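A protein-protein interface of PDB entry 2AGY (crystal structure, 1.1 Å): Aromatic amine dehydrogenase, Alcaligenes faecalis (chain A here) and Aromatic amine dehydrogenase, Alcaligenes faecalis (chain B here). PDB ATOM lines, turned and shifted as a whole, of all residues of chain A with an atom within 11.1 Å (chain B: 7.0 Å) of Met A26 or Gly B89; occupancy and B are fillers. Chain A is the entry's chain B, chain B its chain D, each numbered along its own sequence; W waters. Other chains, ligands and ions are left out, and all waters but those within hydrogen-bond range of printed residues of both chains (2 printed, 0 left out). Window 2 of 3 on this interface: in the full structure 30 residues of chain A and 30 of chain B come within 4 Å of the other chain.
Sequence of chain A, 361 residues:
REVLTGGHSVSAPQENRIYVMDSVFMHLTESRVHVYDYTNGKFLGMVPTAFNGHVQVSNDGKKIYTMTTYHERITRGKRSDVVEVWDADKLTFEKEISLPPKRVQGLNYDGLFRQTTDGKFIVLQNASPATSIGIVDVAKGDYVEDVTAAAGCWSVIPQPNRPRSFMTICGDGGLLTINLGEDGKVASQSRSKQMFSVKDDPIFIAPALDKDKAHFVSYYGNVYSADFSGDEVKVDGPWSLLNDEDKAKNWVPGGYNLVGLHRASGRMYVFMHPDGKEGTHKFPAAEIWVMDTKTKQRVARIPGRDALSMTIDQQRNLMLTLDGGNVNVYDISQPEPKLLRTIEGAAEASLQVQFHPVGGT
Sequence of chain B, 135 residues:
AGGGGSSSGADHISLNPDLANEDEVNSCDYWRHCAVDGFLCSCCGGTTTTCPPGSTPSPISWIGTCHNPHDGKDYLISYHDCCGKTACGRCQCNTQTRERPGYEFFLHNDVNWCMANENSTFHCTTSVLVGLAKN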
ATOM      1  N   MET A  21      -8.556  27.103  27.309  1.00  0.00           N
ATOM      2  CA  MET A  21      -9.990  27.119  27.299  1.00  0.00           C
ATOM      3  C   MET A  21     -10.453  25.990  26.402  1.00  0.00           C
ATOM      4  O   MET A  21     -10.364  26.089  25.187  1.00  0.00           O
ATOM      5  CB  MET A  21     -10.483  28.481  26.776  1.00  0.00           C
ATOM      6  CG  MET A  21     -11.982  28.629  26.746  1.00  0.00           C
ATOM      7  SD  MET A  21     -12.804  28.468  28.361  1.00  0.00           S
ATOM      8  CE  MET A  21     -13.904  27.067  28.028  1.00  0.00           C
ATOM      9  N   ASP A  22     -10.934  24.908  26.999  1.00  0.00           N
ATOM     10  CA  ASP A  22     -11.355  23.758  26.214  1.00  0.00           C
ATOM     11  C   ASP A  22     -12.834  23.856  25.928  1.00  0.00           C
ATOM     12  O   ASP A  22     -13.660  23.655  26.805  1.00  0.00           O
ATOM     13  CB  ASP A  22     -11.013  22.454  26.924  1.00  0.00           C
ATOM     14  CG  ASP A  22     -11.073  21.272  26.010  1.00  0.00           C
ATOM     15  OD1 ASP A  22     -11.526  21.420  24.831  1.00  0.00           O
ATOM     16  OD2 ASP A  22     -10.653  20.150  26.438  1.00  0.00           O
ATOM     17  N   SER A  23     -13.176  24.186  24.687  1.00  0.00           N
ATOM     18  CA  SER A  23     -14.577  24.233  24.304  1.00  0.00           C
ATOM     19  C   SER A  23     -15.254  22.879  24.388  1.00  0.00           C
ATOM     20  O   SER A  23     -16.457  22.813  24.563  1.00  0.00           O
ATOM     21  CB  SER A  23     -14.733  24.799  22.897  1.00  0.00           C
ATOM     22  OG  SER A  23     -14.413  23.843  21.886  1.00  0.00           O
ATOM     23  N   VAL A  24     -14.494  21.803  24.235  1.00  0.00           N
ATOM     24  CA  VAL A  24     -15.076  20.467  24.162  1.00  0.00           C
ATOM     25  C   VAL A  24     -16.268  20.494  23.200  1.00  0.00           C
ATOM     26  O   VAL A  24     -17.386  20.108  23.540  1.00  0.00           O
ATOM     27  CB  VAL A  24     -15.500  19.919  25.554  1.00  0.00           C
ATOM     28  CG1 VAL A  24     -15.768  18.434  25.470  1.00  0.00           C
ATOM     29  CG2 VAL A  24     -14.430  20.190  26.571  1.00  0.00           C
ATOM     30  N   PHE A  25     -16.037  20.944  21.983  1.00  0.00           N
ATOM     31  CA  PHE A  25     -17.114  21.151  21.035  1.00  0.00           C
ATOM     32  C   PHE A  25     -17.973  19.903  20.832  1.00  0.00           C
ATOM     33  O   PHE A  25     -19.159  20.003  20.627  1.00  0.00           O
ATOM     34  CB  PHE A  25     -16.545  21.637  19.694  1.00  0.00           C
ATOM     35  CG  PHE A  25     -17.569  22.173  18.766  1.00  0.00           C
ATOM     36  CD1 PHE A  25     -18.101  23.433  18.959  1.00  0.00           C
ATOM     37  CD2 PHE A  25     -18.012  21.418  17.700  1.00  0.00           C
ATOM     38  CE1 PHE A  25     -19.066  23.931  18.080  1.00  0.00           C
ATOM     39  CE2 PHE A  25     -18.949  21.900  16.851  1.00  0.00           C
ATOM     40  CZ  PHE A  25     -19.476  23.155  17.033  1.00  0.00           C
ATOM     41  N   MET A  26     -17.382  18.725  20.879  1.00  0.00           N
ATOM     42  CA  MET A  26     -18.139  17.498  20.750  1.00  0.00           C
ATOM     43  C   MET A  26     -19.155  17.299  21.877  1.00  0.00           C
ATOM     44  O   MET A  26     -20.124  16.577  21.725  1.00  0.00           O
ATOM     45  CB  MET A  26     -17.199  16.312  20.708  1.00  0.00           C
ATOM     46  CG  MET A  26     -16.442  16.168  19.414  1.00  0.00           C
ATOM     47  SD  MET A  26     -17.476  15.649  18.033  1.00  0.00           S
ATOM     48  CE  MET A  26     -17.867  13.971  18.561  1.00  0.00           C
ATOM     49  N   HIS A  27     -18.898  17.954  23.013  1.00  0.00           N
ATOM     50  CA  HIS A  27     -19.785  17.936  24.189  1.00  0.00           C
ATOM     51  C   HIS A  27     -19.775  19.296  24.818  1.00  0.00           C
ATOM     52  O   HIS A  27     -19.352  19.481  25.942  1.00  0.00           O
ATOM     53  CB  HIS A  27     -19.378  16.823  25.166  1.00  0.00           C
ATOM     54  CG  HIS A  27     -19.438  15.494  24.524  1.00  0.00           C
ATOM     55  ND1 HIS A  27     -20.635  14.900  24.189  1.00  0.00           N
ATOM     56  CD2 HIS A  27     -18.472  14.667  24.084  1.00  0.00           C
ATOM     57  CE1 HIS A  27     -20.395  13.746  23.590  1.00  0.00           C
ATOM     58  NE2 HIS A  27     -19.086  13.582  23.512  1.00  0.00           N
ATOM     59  N   LEU A  28     -20.276  20.269  24.045  1.00  0.00           N
ATOM     60  CA  LEU A  28     -20.052  21.666  24.303  1.00  0.00           C
ATOM     61  C   LEU A  28     -20.716  22.154  25.591  1.00  0.00           C
ATOM     62  O   LEU A  28     -20.378  23.214  26.079  1.00  0.00           O
ATOM     63  CB  LEU A  28     -20.537  22.471  23.094  1.00  0.00           C
ATOM     64  CG  LEU A  28     -20.309  23.974  23.063  1.00  0.00           C
ATOM     65  CD1 LEU A  28     -18.843  24.348  23.247  1.00  0.00           C
ATOM     66  CD2 LEU A  28     -20.817  24.516  21.756  1.00  0.00           C
ATOM     67  N   THR A  29     -21.666  21.392  26.127  1.00  0.00           N
ATOM     68  CA  THR A  29     -22.236  21.746  27.422  1.00  0.00           C
ATOM     69  C   THR A  29     -21.297  21.445  28.593  1.00  0.00           C
ATOM     70  O   THR A  29     -21.628  21.772  29.712  1.00  0.00           O
ATOM     71  CB  THR A  29     -23.580  21.049  27.705  1.00  0.00           C
ATOM     72  OG1 THR A  29     -23.382  19.618  27.784  1.00  0.00           O
ATOM     73  CG2 THR A  29     -24.643  21.351  26.660  1.00  0.00           C
ATOM     74  N   GLU A  30     -20.145  20.826  28.332  1.00  0.00           N
ATOM     75  CA  GLU A  30     -19.174  20.525  29.386  1.00  0.00           C
ATOM     76  C   GLU A  30     -17.792  21.114  29.067  1.00  0.00           C
ATOM     77  O   GLU A  30     -16.754  20.515  29.318  1.00  0.00           O
ATOM     78  CB  GLU A  30     -19.091  19.029  29.693  1.00  0.00           C
ATOM     79  CG  GLU A  30     -18.634  18.775  31.139  1.00  0.00           C
ATOM     80  CD  GLU A  30     -18.300  17.339  31.398  1.00  0.00           C
ATOM     81  OE1 GLU A  30     -19.196  16.566  31.783  1.00  0.00           O
ATOM     82  OE2 GLU A  30     -17.118  16.962  31.241  1.00  0.00           O
ATOM     83  N   SER A  31     -17.814  22.302  28.494  1.00  0.00           N
ATOM     84  CA  SER A  31     -16.602  23.055  28.310  1.00  0.00           C
ATOM     85  C   SER A  31     -15.954  23.333  29.666  1.00  0.00           C
ATOM     86  O   SER A  31     -16.605  23.305  30.700  1.00  0.00           O
ATOM     87  CB  SER A  31     -16.880  24.373  27.566  1.00  0.00           C
ATOM     88  OG  SER A  31     -17.589  25.320  28.368  1.00  0.00           O
ATOM     89  N   ARG A  32     -14.657  23.595  29.651  1.00  0.00           N
ATOM     90  CA  ARG A  32     -13.938  23.861  30.875  1.00  0.00           C
ATOM     91  C   ARG A  32     -12.633  24.534  30.580  1.00  0.00           C
ATOM     92  O   ARG A  32     -12.132  24.482  29.468  1.00  0.00           O
ATOM     93  CB  ARG A  32     -13.690  22.564  31.655  1.00  0.00           C
ATOM     94  CG  ARG A  32     -12.624  21.636  31.062  1.00  0.00           C
ATOM     95  CD  ARG A  32     -13.146  20.667  29.983  1.00  0.00           C
ATOM     96  NE  ARG A  32     -14.067  19.707  30.567  1.00  0.00           N
ATOM     97  CZ  ARG A  32     -13.669  18.695  31.337  1.00  0.00           C
ATOM     98  NH1 ARG A  32     -12.383  18.496  31.577  1.00  0.00           N
ATOM     99  NH2 ARG A  32     -14.560  17.873  31.864  1.00  0.00           N
ATOM    100  N   ALA A  50     -19.618  24.916  31.736  1.00  0.00           N
ATOM    101  CA  ALA A  50     -20.924  24.652  31.156  1.00  0.00           C
ATOM    102  C   ALA A  50     -20.919  24.837  29.631  1.00  0.00           C
ATOM    103  O   ALA A  50     -20.010  24.352  28.957  1.00  0.00           O
ATOM    104  CB  ALA A  50     -21.977  25.502  31.853  1.00  0.00           C
ATOM    105  N   PHE A  51     -21.929  25.490  29.072  1.00  0.00           N
ATOM    106  CA  PHE A  51     -22.047  25.542  27.628  1.00  0.00           C
ATOM    107  C   PHE A  51     -21.195  26.643  27.056  1.00  0.00           C
ATOM    108  O   PHE A  51     -21.439  27.822  27.328  1.00  0.00           O
ATOM    109  CB  PHE A  51     -23.498  25.758  27.212  1.00  0.00           C
ATOM    110  CG  PHE A  51     -23.696  25.834  25.728  1.00  0.00           C
ATOM    111  CD1 PHE A  51     -23.677  24.701  24.963  1.00  0.00           C
ATOM    112  CD2 PHE A  51     -23.926  27.033  25.104  1.00  0.00           C
ATOM    113  CE1 PHE A  51     -23.867  24.769  23.597  1.00  0.00           C
ATOM    114  CE2 PHE A  51     -24.109  27.095  23.743  1.00  0.00           C
ATOM    115  CZ  PHE A  51     -24.084  25.967  23.001  1.00  0.00           C
ATOM    116  N   ASN A  52     -20.221  26.274  26.239  1.00  0.00           N
ATOM    117  CA  ASN A  52     -19.418  27.247  25.493  1.00  0.00           C
ATOM    118  C   ASN A  52     -18.874  28.350  26.387  1.00  0.00           C
ATOM    119  O   ASN A  52     -19.115  29.515  26.166  1.00  0.00           O
ATOM    120  CB  ASN A  52     -20.232  27.838  24.350  1.00  0.00           C
ATOM    121  CG  ASN A  52     -19.452  28.851  23.538  1.00  0.00           C
ATOM    122  OD1 ASN A  52     -18.248  28.643  23.197  1.00  0.00           O
ATOM    123  ND2 ASN A  52     -20.091  29.922  23.205  1.00  0.00           N
ATOM    124  N   LEU A 107     -16.936  30.752  19.170  1.00  0.00           N
ATOM    125  CA  LEU A 107     -15.571  30.325  19.424  1.00  0.00           C
ATOM    126  C   LEU A 107     -14.794  31.369  20.207  1.00  0.00           C
ATOM    127  O   LEU A 107     -15.141  32.562  20.205  1.00  0.00           O
ATOM    128  CB  LEU A 107     -14.873  30.022  18.088  1.00  0.00           C
ATOM    129  CG  LEU A 107     -15.569  28.970  17.211  1.00  0.00           C
ATOM    130  CD1 LEU A 107     -14.758  28.712  16.002  1.00  0.00           C
ATOM    131  CD2 LEU A 107     -15.883  27.668  17.956  1.00  0.00           C
ATOM    132  N   ASN A 108     -13.732  30.908  20.878  1.00  0.00           N
ATOM    133  CA  ASN A 108     -13.073  31.684  21.901  1.00  0.00           C
ATOM    134  C   ASN A 108     -11.997  32.657  21.413  1.00  0.00           C
ATOM    135  O   ASN A 108     -10.823  32.557  21.788  1.00  0.00           O
ATOM    136  CB  ASN A 108     -12.470  30.744  22.934  1.00  0.00           C
ATOM    137  CG  ASN A 108     -13.531  30.024  23.753  1.00  0.00           C
ATOM    138  OD1 ASN A 108     -14.097  30.596  24.710  1.00  0.00           O
ATOM    139  ND2 ASN A 108     -13.813  28.802  23.396  1.00  0.00           N
ATOM    140  N   GLY A 324      -5.255  23.242  18.806  1.00  0.00           N
ATOM    141  CA  GLY A 324      -6.539  22.647  19.148  1.00  0.00           C
ATOM    142  C   GLY A 324      -6.449  21.717  20.323  1.00  0.00           C
ATOM    143  O   GLY A 324      -7.393  21.597  21.102  1.00  0.00           O
ATOM    144  N   ALA A 347      -6.031  19.917  25.737  1.00  0.00           N
ATOM    145  CA  ALA A 347      -7.444  20.129  25.478  1.00  0.00           C
ATOM    146  C   ALA A 347      -7.881  19.205  24.398  1.00  0.00           C
ATOM    147  O   ALA A 347      -7.070  18.702  23.636  1.00  0.00           O
ATOM    148  CB  ALA A 347      -7.691  21.563  25.015  1.00  0.00           C
ATOM    149  N   GLU A 348      -9.187  18.991  24.312  1.00  0.00           N
ATOM    150  CA  GLU A 348      -9.775  18.324  23.167  1.00  0.00           C
ATOM    151  C   GLU A 348     -10.092  19.262  22.019  1.00  0.00           C
ATOM    152  O   GLU A 348      -9.940  18.895  20.859  1.00  0.00           O
ATOM    153  CB  GLU A 348     -11.023  17.580  23.577  1.00  0.00           C
ATOM    154  CG  GLU A 348     -10.691  16.403  24.447  1.00  0.00           C
ATOM    155  CD  GLU A 348     -11.918  15.701  24.903  1.00  0.00           C
ATOM    156  OE1 GLU A 348     -12.396  14.805  24.190  1.00  0.00           O
ATOM    157  OE2 GLU A 348     -12.405  16.050  25.954  1.00  0.00           O
ATOM    158  N   ALA A 349     -10.538  20.471  22.341  1.00  0.00           N
ATOM    159  CA  ALA A 349     -10.936  21.428  21.317  1.00  0.00           C
ATOM    160  C   ALA A 349     -10.789  22.827  21.850  1.00  0.00           C
ATOM    161  O   ALA A 349     -11.765  23.475  22.229  1.00  0.00           O
ATOM    162  CB  ALA A 349     -12.383  21.180  20.868  1.00  0.00           C
ATOM    163  N   SER A 350      -9.564  23.321  21.861  1.00  0.00           N
ATOM    164  CA  SER A 350      -9.281  24.658  22.351  1.00  0.00           C
ATOM    165  C   SER A 350      -8.734  25.534  21.265  1.00  0.00           C
ATOM    166  O   SER A 350      -7.832  25.145  20.541  1.00  0.00           O
ATOM    167  CB  SER A 350      -8.258  24.616  23.466  1.00  0.00           C
ATOM    168  OG  SER A 350      -7.991  25.928  23.939  1.00  0.00           O
ATOM    169  N   PHE B  39     -21.983  20.230  12.671  1.00  0.00           N
ATOM    170  CA  PHE B  39     -22.243  18.844  12.319  1.00  0.00           C
ATOM    171  C   PHE B  39     -23.328  18.822  11.286  1.00  0.00           C
ATOM    172  O   PHE B  39     -24.339  19.488  11.435  1.00  0.00           O
ATOM    173  CB  PHE B  39     -22.731  18.071  13.552  1.00  0.00           C
ATOM    174  CG  PHE B  39     -21.826  18.206  14.734  1.00  0.00           C
ATOM    175  CD1 PHE B  39     -22.211  18.938  15.857  1.00  0.00           C
ATOM    176  CD2 PHE B  39     -20.585  17.628  14.718  1.00  0.00           C
ATOM    177  CE1 PHE B  39     -21.376  19.067  16.925  1.00  0.00           C
ATOM    178  CE2 PHE B  39     -19.738  17.758  15.796  1.00  0.00           C
ATOM    179  CZ  PHE B  39     -20.141  18.479  16.898  1.00  0.00           C
ATOM    180  N   CYS B  44     -27.287  13.200  11.203  1.00  0.00           N
ATOM    181  CA  CYS B  44     -27.737  13.285  12.597  1.00  0.00           C
ATOM    182  C   CYS B  44     -29.204  12.903  12.718  1.00  0.00           C
ATOM    183  O   CYS B  44     -29.847  13.216  13.695  1.00  0.00           O
ATOM    184  CB  CYS B  44     -27.524  14.708  13.105  1.00  0.00           C
ATOM    185  SG  CYS B  44     -25.772  15.182  13.105  1.00  0.00           S
ATOM    186  N   THR B  86     -28.217  18.365  22.531  1.00  0.00           N
ATOM    187  CA  THR B  86     -26.774  18.431  22.652  1.00  0.00           C
ATOM    188  C   THR B  86     -26.112  17.952  21.353  1.00  0.00           C
ATOM    189  O   THR B  86     -26.761  17.376  20.454  1.00  0.00           O
ATOM    190  CB  THR B  86     -26.317  17.641  23.865  1.00  0.00           C
ATOM    191  OG1 THR B  86     -27.008  16.389  23.876  1.00  0.00           O
ATOM    192  CG2 THR B  86     -26.681  18.384  25.137  1.00  0.00           C
ATOM    193  N   ALA B  87     -24.818  18.207  21.262  1.00  0.00           N
ATOM    194  CA  ALA B  87     -24.087  18.099  20.024  1.00  0.00           C
ATOM    195  C   ALA B  87     -24.263  16.750  19.357  1.00  0.00           C
ATOM    196  O   ALA B  87     -24.050  15.704  19.967  1.00  0.00           O
ATOM    197  CB  ALA B  87     -22.617  18.308  20.325  1.00  0.00           C
ATOM    198  N   CYS B  88     -24.617  16.756  18.084  1.00  0.00           N
ATOM    199  CA  CYS B  88     -24.774  15.523  17.373  1.00  0.00           C
ATOM    200  C   CYS B  88     -23.478  14.728  17.271  1.00  0.00           C
ATOM    201  O   CYS B  88     -23.479  13.507  17.411  1.00  0.00           O
ATOM    202  CB  CYS B  88     -25.276  15.810  15.983  1.00  0.00           C
ATOM    203  SG  CYS B  88     -25.164  14.413  14.872  1.00  0.00           S
ATOM    204  N   GLY B  89     -22.378  15.420  17.011  1.00  0.00           N
ATOM    205  CA  GLY B  89     -21.077  14.797  17.007  1.00  0.00           C
ATOM    206  C   GLY B  89     -20.683  14.096  15.727  1.00  0.00           C
ATOM    207  O   GLY B  89     -19.580  13.637  15.626  1.00  0.00           O
ATOM    208  N   ARG B  90     -21.567  14.010  14.754  1.00  0.00           N
ATOM    209  CA  ARG B  90     -21.273  13.312  13.512  1.00  0.00           C
ATOM    210  C   ARG B  90     -21.070  14.277  12.389  1.00  0.00           C
ATOM    211  O   ARG B  90     -21.724  15.313  12.330  1.00  0.00           O
ATOM    212  CB  ARG B  90     -22.416  12.353  13.204  1.00  0.00           C
ATOM    213  CG  ARG B  90     -22.421  11.214  14.172  1.00  0.00           C
ATOM    214  CD  ARG B  90     -23.713  10.814  14.698  1.00  0.00           C
ATOM    215  NE  ARG B  90     -23.557   9.611  15.526  1.00  0.00           N
ATOM    216  CZ  ARG B  90     -23.172   9.573  16.813  1.00  0.00           C
ATOM    217  NH1 ARG B  90     -22.885  10.679  17.498  1.00  0.00           N
ATOM    218  NH2 ARG B  90     -23.075   8.401  17.406  1.00  0.00           N
ATOM    219  N   CYS B  91     -20.155  13.930  11.480  1.00  0.00           N
ATOM    220  CA  CYS B  91     -19.924  14.724  10.261  1.00  0.00           C
ATOM    221  C   CYS B  91     -19.643  16.167  10.597  1.00  0.00           C
ATOM    222  O   CYS B  91     -20.306  17.078  10.118  1.00  0.00           O
ATOM    223  CB  CYS B  91     -21.112  14.635   9.308  1.00  0.00           C
ATOM    224  SG  CYS B  91     -21.438  12.990   8.718  1.00  0.00           S
ATOM    225  N   GLN B  92     -18.650  16.386  11.431  1.00  0.00           N
ATOM    226  CA  GLN B  92     -18.212  17.731  11.712  1.00  0.00           C
ATOM    227  C   GLN B  92     -17.518  18.307  10.506  1.00  0.00           C
ATOM    228  O   GLN B  92     -16.632  17.676   9.930  1.00  0.00           O
ATOM    229  CB  GLN B  92     -17.283  17.792  12.910  1.00  0.00           C
ATOM    230  CG  GLN B  92     -17.039  19.214  13.335  1.00  0.00           C
ATOM    231  CD  GLN B  92     -16.241  19.359  14.606  1.00  0.00           C
ATOM    232  OE1 GLN B  92     -15.863  20.479  14.976  1.00  0.00           O
ATOM    233  NE2 GLN B  92     -15.984  18.268  15.270  1.00  0.00           N
ATOM    234  N   HIS B 123     -27.172  21.606  18.096  1.00  0.00           N
ATOM    235  CA  HIS B 123     -27.261  20.216  17.737  1.00  0.00           C
ATOM    236  C   HIS B 123     -26.564  19.884  16.416  1.00  0.00           C
ATOM    237  O   HIS B 123     -25.680  19.009  16.373  1.00  0.00           O
ATOM    238  CB  HIS B 123     -28.712  19.775  17.722  1.00  0.00           C
ATOM    239  CG  HIS B 123     -28.892  18.329  17.461  1.00  0.00           C
ATOM    240  ND1 HIS B 123     -28.299  17.347  18.209  1.00  0.00           N
ATOM    241  CD2 HIS B 123     -29.628  17.691  16.519  1.00  0.00           C
ATOM    242  CE1 HIS B 123     -28.654  16.160  17.724  1.00  0.00           C
ATOM    243  NE2 HIS B 123     -29.464  16.345  16.699  1.00  0.00           N
ATOM    244  N   CYS B 124     -26.953  20.563  15.350  1.00  0.00           N
ATOM    245  CA  CYS B 124     -26.363  20.338  14.052  1.00  0.00           C
ATOM    246  C   CYS B 124     -26.707  21.500  13.149  1.00  0.00           C
ATOM    247  O   CYS B 124     -27.495  22.371  13.522  1.00  0.00           O
ATOM    248  CB  CYS B 124     -26.820  19.005  13.448  1.00  0.00           C
ATOM    249  SG  CYS B 124     -28.592  18.844  13.126  1.00  0.00           S
HETATM  250  O   HOH W   1     -21.360  14.621  20.224  1.00  0.00           O
HETATM  251  O   HOH W   2     -15.490  15.742  14.954  1.00  0.00           O
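Along chain A the printed residues that touch a printed residue of chain B span positions 25 to 29.
Of the 11 printed residues of chain B, 5 touch a printed residue of chain A.
Printed residues of chain B that touch a printed residue of chain A: Phe B39, Thr B86, Ala B87, Gly B89 and Gln B92.
Hydrophobic or aromatic side chains of chain B that line the printed part of chain A: Phe B39 and Ala B87.
Along chain B the printed residues that touch a printed residue of chain A span positions 39 to 92.
Among the printed residues, 7 pairs touch across the chains.
Among the printed residues, no Asp or Glu carboxylate lies within 4 Å of a Lys or Arg side-chain nitrogen of the other chain.
Phe B39 touches Phe A25 (CZ to CE2, 3.6 Å).
Ala B87 touches Phe A25 (CB to O, 3.9 Å).
Gln B92 touches Phe A25 (OE1 to CD2, 3.6 Å).
CE2 of Phe B39 touches SD of Met A26 (3.8 Å).
Met A26 touches Ala B87 (O to CB, 3.3 Å).
Thr A29 touches Thr B86.
O of Thr B86 sits at hydrogen-bond distance from ND1 of His B123 (2.7 Å).
The side-chain hydroxyl (OG) of Ser A23 sits close to the backbone NH (N) of Phe A25 (3.3 Å).
The side-chain sulfur (SG) of Cys B88 forms a disulfide with the side-chain sulfur (SG) of Cys B44 (2.0 Å).
Water W2 lies within hydrogen-bond range of NE2 of Gln B92 (2.6 Å) and SD of Met A26 (3.7 Å).
Water W1 lies within hydrogen-bond range of O of Met A26, O of Ala B87 and N of Gly B89.
Met A26 touches just these residues of chain B: Phe B39 (3.8 Å), Ala B87 (3.3 Å) and Gly B89 (3.4 Å).
Gly B89 touches just one residue of chain A: Met A26 (3.4 Å).
Of the printed residues of chain A, Ala B87 touches Phe A25 and Met A26.
No residue of chain A comes within 4 Å of Cys B88.
No residue of chain A comes within 4 Å of Arg B90.
Of the printed residues of chain B, Thr A29 touches Thr B86.
Printed residues of chain A within 4 Å of Thr B86: Thr A29 (3.9 Å).
Of the printed residues of chain A, Phe B39 touches Phe A25 and Met A26.
Printed residues of chain A within 4 Å of Gln B92: Phe A25.
Asn A52 touches none of the printed residues of chain B.
Met A21 touches none of the printed residues of chain B.
The nearest residue of chain B that does not touch Met A26 is Gln B92 (4.1 Å).
The nearest printed residue of chain A that does not touch Gln B92 is Met A26 (4.1 Å).
The side-chain sulfur of Met A26 lies close to the backbone carbonyl oxygen of Gly B89, 3.8 Å away.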
